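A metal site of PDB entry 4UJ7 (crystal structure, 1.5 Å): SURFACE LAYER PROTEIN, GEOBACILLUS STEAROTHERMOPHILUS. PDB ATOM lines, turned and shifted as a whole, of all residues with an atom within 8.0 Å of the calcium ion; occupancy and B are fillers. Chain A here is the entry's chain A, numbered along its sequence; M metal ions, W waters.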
ATOM      1  N   SER A 161     -27.528 -27.784  -8.028  1.00  0.00           N
ATOM      2  CA  SER A 161     -26.436 -26.974  -7.517  1.00  0.00           C
ATOM      3  C   SER A 161     -27.019 -25.704  -6.909  1.00  0.00           C
ATOM      4  O   SER A 161     -28.225 -25.449  -7.024  1.00  0.00           O
ATOM      5  CB  SER A 161     -25.490 -26.606  -8.646  1.00  0.00           C
ATOM      6  OG  SER A 161     -26.171 -25.864  -9.654  1.00  0.00           O
ATOM      7  N   GLU A 162     -26.157 -24.870  -6.331  1.00  0.00           N
ATOM      8  CA  GLU A 162     -26.603 -23.605  -5.755  1.00  0.00           C
ATOM      9  C   GLU A 162     -27.446 -22.781  -6.745  1.00  0.00           C
ATOM     10  O   GLU A 162     -27.145 -22.715  -7.940  1.00  0.00           O
ATOM     11  CB  GLU A 162     -25.419 -22.776  -5.235  1.00  0.00           C
ATOM     12  CG  GLU A 162     -24.378 -22.460  -6.301  1.00  0.00           C
ATOM     13  CD  GLU A 162     -23.180 -21.681  -5.812  1.00  0.00           C
ATOM     14  OE1 GLU A 162     -23.150 -21.304  -4.606  1.00  0.00           O
ATOM     15  OE2 GLU A 162     -22.265 -21.446  -6.625  1.00  0.00           O
ATOM     16  N   ALA A 163     -28.517 -22.180  -6.240  1.00  0.00           N
ATOM     17  CA  ALA A 163     -29.452 -21.410  -7.060  1.00  0.00           C
ATOM     18  C   ALA A 163     -28.805 -20.175  -7.688  1.00  0.00           C
ATOM     19  O   ALA A 163     -29.104 -19.836  -8.825  1.00  0.00           O
ATOM     20  CB  ALA A 163     -30.669 -21.012  -6.226  1.00  0.00           C
ATOM     21  N   THR A 164     -27.947 -19.504  -6.935  1.00  0.00           N
ATOM     22  CA  THR A 164     -27.221 -18.305  -7.370  1.00  0.00           C
ATOM     23  C   THR A 164     -25.738 -18.690  -7.327  1.00  0.00           C
ATOM     24  O   THR A 164     -25.264 -19.205  -6.298  1.00  0.00           O
ATOM     25  CB  THR A 164     -27.484 -17.173  -6.353  1.00  0.00           C
ATOM     26  OG1 THR A 164     -28.860 -16.788  -6.434  1.00  0.00           O
ATOM     27  CG2 THR A 164     -26.605 -15.976  -6.582  1.00  0.00           C
ATOM     28  N   ASP A 165     -24.999 -18.458  -8.405  1.00  0.00           N
ATOM     29  CA  ASP A 165     -23.573 -18.790  -8.423  1.00  0.00           C
ATOM     30  C   ASP A 165     -22.770 -17.923  -7.485  1.00  0.00           C
ATOM     31  O   ASP A 165     -22.925 -16.696  -7.476  1.00  0.00           O
ATOM     32  CB  ASP A 165     -22.953 -18.663  -9.823  1.00  0.00           C
ATOM     33  CG  ASP A 165     -21.479 -18.946  -9.810  1.00  0.00           C
ATOM     34  OD1 ASP A 165     -21.095 -20.016  -9.288  1.00  0.00           O
ATOM     35  OD2 ASP A 165     -20.678 -18.114 -10.271  1.00  0.00           O
ATOM     36  N   THR A 166     -21.911 -18.551  -6.681  1.00  0.00           N
ATOM     37  CA  THR A 166     -21.073 -17.802  -5.733  1.00  0.00           C
ATOM     38  C   THR A 166     -19.592 -18.106  -5.870  1.00  0.00           C
ATOM     39  O   THR A 166     -18.783 -17.607  -5.060  1.00  0.00           O
ATOM     40  CB  THR A 166     -21.523 -18.040  -4.257  1.00  0.00           C
ATOM     41  OG1 THR A 166     -21.233 -19.403  -3.882  1.00  0.00           O
ATOM     42  CG2 THR A 166     -23.012 -17.721  -4.005  1.00  0.00           C
ATOM     43  N   ASN A 167     -19.214 -18.927  -6.865  1.00  0.00           N
ATOM     44  CA  ASN A 167     -17.826 -19.354  -7.038  1.00  0.00           C
ATOM     45  C   ASN A 167     -17.299 -19.418  -8.478  1.00  0.00           C
ATOM     46  O   ASN A 167     -16.164 -19.855  -8.708  1.00  0.00           O
ATOM     47  CB  ASN A 167     -17.582 -20.702  -6.326  1.00  0.00           C
ATOM     48  CG  ASN A 167     -18.321 -21.850  -6.980  1.00  0.00           C
ATOM     49  OD1 ASN A 167     -19.246 -21.644  -7.753  1.00  0.00           O
ATOM     50  ND2 ASN A 167     -17.888 -23.075  -6.689  1.00  0.00           N
ATOM     51  N   GLY A 168     -18.097 -18.988  -9.459  1.00  0.00           N
ATOM     52  CA  GLY A 168     -17.634 -18.999 -10.861  1.00  0.00           C
ATOM     53  C   GLY A 168     -17.628 -20.370 -11.539  1.00  0.00           C
ATOM     54  O   GLY A 168     -17.146 -20.502 -12.663  1.00  0.00           O
ATOM     55  N   VAL A 169     -18.130 -21.388 -10.835  1.00  0.00           N
ATOM     56  CA  VAL A 169     -18.267 -22.740 -11.391  1.00  0.00           C
ATOM     57  C   VAL A 169     -19.749 -23.001 -11.543  1.00  0.00           C
ATOM     58  O   VAL A 169     -20.490 -22.973 -10.554  1.00  0.00           O
ATOM     59  CB  VAL A 169     -17.635 -23.808 -10.469  1.00  0.00           C
ATOM     60  CG1 VAL A 169     -17.687 -25.196 -11.106  1.00  0.00           C
ATOM     61  CG2 VAL A 169     -16.187 -23.449 -10.155  1.00  0.00           C
ATOM     62  N   ILE A 170     -20.173 -23.246 -12.773  1.00  0.00           N
ATOM     63  CA  ILE A 170     -21.592 -23.314 -13.092  1.00  0.00           C
ATOM     64  C   ILE A 170     -21.840 -24.564 -13.936  1.00  0.00           C
ATOM     65  O   ILE A 170     -21.223 -24.724 -15.015  1.00  0.00           O
ATOM     66  CB  ILE A 170     -22.103 -22.034 -13.797  1.00  0.00           C
ATOM     67  CG1 ILE A 170     -21.587 -20.790 -13.050  1.00  0.00           C
ATOM     68  CG2 ILE A 170     -23.622 -22.043 -13.843  1.00  0.00           C
ATOM     69  CD1 ILE A 170     -21.687 -19.501 -13.847  1.00  0.00           C
ATOM     70  N   VAL A 171     -22.730 -25.432 -13.445  1.00  0.00           N
ATOM     71  CA  VAL A 171     -23.034 -26.680 -14.162  1.00  0.00           C
ATOM     72  C   VAL A 171     -24.526 -26.915 -14.302  1.00  0.00           C
ATOM     73  O   VAL A 171     -25.321 -26.370 -13.523  1.00  0.00           O
ATOM     74  CB  VAL A 171     -22.395 -27.917 -13.474  1.00  0.00           C
ATOM     75  CG1 VAL A 171     -20.881 -27.808 -13.447  1.00  0.00           C
ATOM     76  CG2 VAL A 171     -22.933 -28.120 -12.068  1.00  0.00           C
ATOM     77  N   SER A 191     -18.999 -21.890 -16.873  1.00  0.00           N
ATOM     78  CA  SER A 191     -18.026 -21.686 -15.792  1.00  0.00           C
ATOM     79  C   SER A 191     -16.927 -20.708 -16.201  1.00  0.00           C
ATOM     80  O   SER A 191     -16.367 -20.840 -17.287  1.00  0.00           O
ATOM     81  CB  SER A 191     -17.354 -23.017 -15.405  1.00  0.00           C
ATOM     82  OG  SER A 191     -18.286 -23.896 -14.798  1.00  0.00           O
ATOM     83  N   LYS A 196     -14.401 -26.827  -7.251  1.00  0.00           N
ATOM     84  CA  LYS A 196     -15.465 -27.727  -6.831  1.00  0.00           C
ATOM     85  C   LYS A 196     -16.824 -27.056  -6.864  1.00  0.00           C
ATOM     86  O   LYS A 196     -16.973 -25.872  -6.503  1.00  0.00           O
ATOM     87  CB  LYS A 196     -15.185 -28.212  -5.389  1.00  0.00           C
ATOM     88  CG  LYS A 196     -13.889 -29.007  -5.185  1.00  0.00           C
ATOM     89  CD  LYS A 196     -13.924 -30.307  -5.975  1.00  0.00           C
ATOM     90  CE  LYS A 196     -12.676 -31.152  -5.803  1.00  0.00           C
ATOM     91  NZ  LYS A 196     -12.723 -31.970  -4.558  1.00  0.00           N
ATOM     92  N   GLU A 197     -17.839 -27.838  -7.247  1.00  0.00           N
ATOM     93  CA  GLU A 197     -19.231 -27.416  -7.144  1.00  0.00           C
ATOM     94  C   GLU A 197     -20.028 -28.476  -6.410  1.00  0.00           C
ATOM     95  O   GLU A 197     -20.040 -29.637  -6.826  1.00  0.00           O
ATOM     96  CB  GLU A 197     -19.802 -27.141  -8.541  1.00  0.00           C
ATOM     97  CG  GLU A 197     -21.233 -26.595  -8.563  1.00  0.00           C
ATOM     98  CD  GLU A 197     -21.355 -25.126  -8.219  1.00  0.00           C
ATOM     99  OE1 GLU A 197     -20.393 -24.516  -7.705  1.00  0.00           O
ATOM    100  OE2 GLU A 197     -22.426 -24.554  -8.512  1.00  0.00           O
ATOM    101  N   THR A 198     -20.680 -28.092  -5.316  1.00  0.00           N
ATOM    102  CA  THR A 198     -21.466 -29.024  -4.499  1.00  0.00           C
ATOM    103  C   THR A 198     -22.836 -29.290  -5.106  1.00  0.00           C
ATOM    104  O   THR A 198     -23.616 -28.354  -5.326  1.00  0.00           O
ATOM    105  CB  THR A 198     -21.606 -28.485  -3.049  1.00  0.00           C
ATOM    106  OG1 THR A 198     -20.293 -28.331  -2.495  1.00  0.00           O
ATOM    107  CG2 THR A 198     -22.389 -29.464  -2.175  1.00  0.00           C
HETATM  108 CA    CA M   1     -21.388 -22.275  -8.570  1.00  0.00          CA
HETATM  109  O   HOH W   1     -23.457 -22.099  -9.800  1.00  0.00           O
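The side-chain carboxylate of Glu 162 lies within hydrogen-bond range of the side-chain hydroxyl of Thr 166. The side-chain amide nitrogen of Asn 167 is in hydrogen-bond range of the backbone carbonyl oxygen of Lys 196, at 2.9 Å. OD2 of Asp 165 is in hydrogen-bond range of N of Gly 168.
Of the 15 residues printed, 5 come within 4 Å of the calcium ion. Along chain A the residues within 4 Å of the calcium ion span positions 162 to 197. The nearest printed residue that does not touch the calcium ion is Thr 166 (4.2 Å).
The calcium ion is bound by the backbone carbonyl oxygen (O) of Val 169, the side-chain carboxylate (OE2) of Glu 162, the side-chain amide oxygen (OD1) of Asn 167, the side-chain carboxylate (OD1) of Asp 165, water W1, the side-chain carboxylate (OE2) of Glu 197 and the side-chain carboxylate (OE1) of Glu 197.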
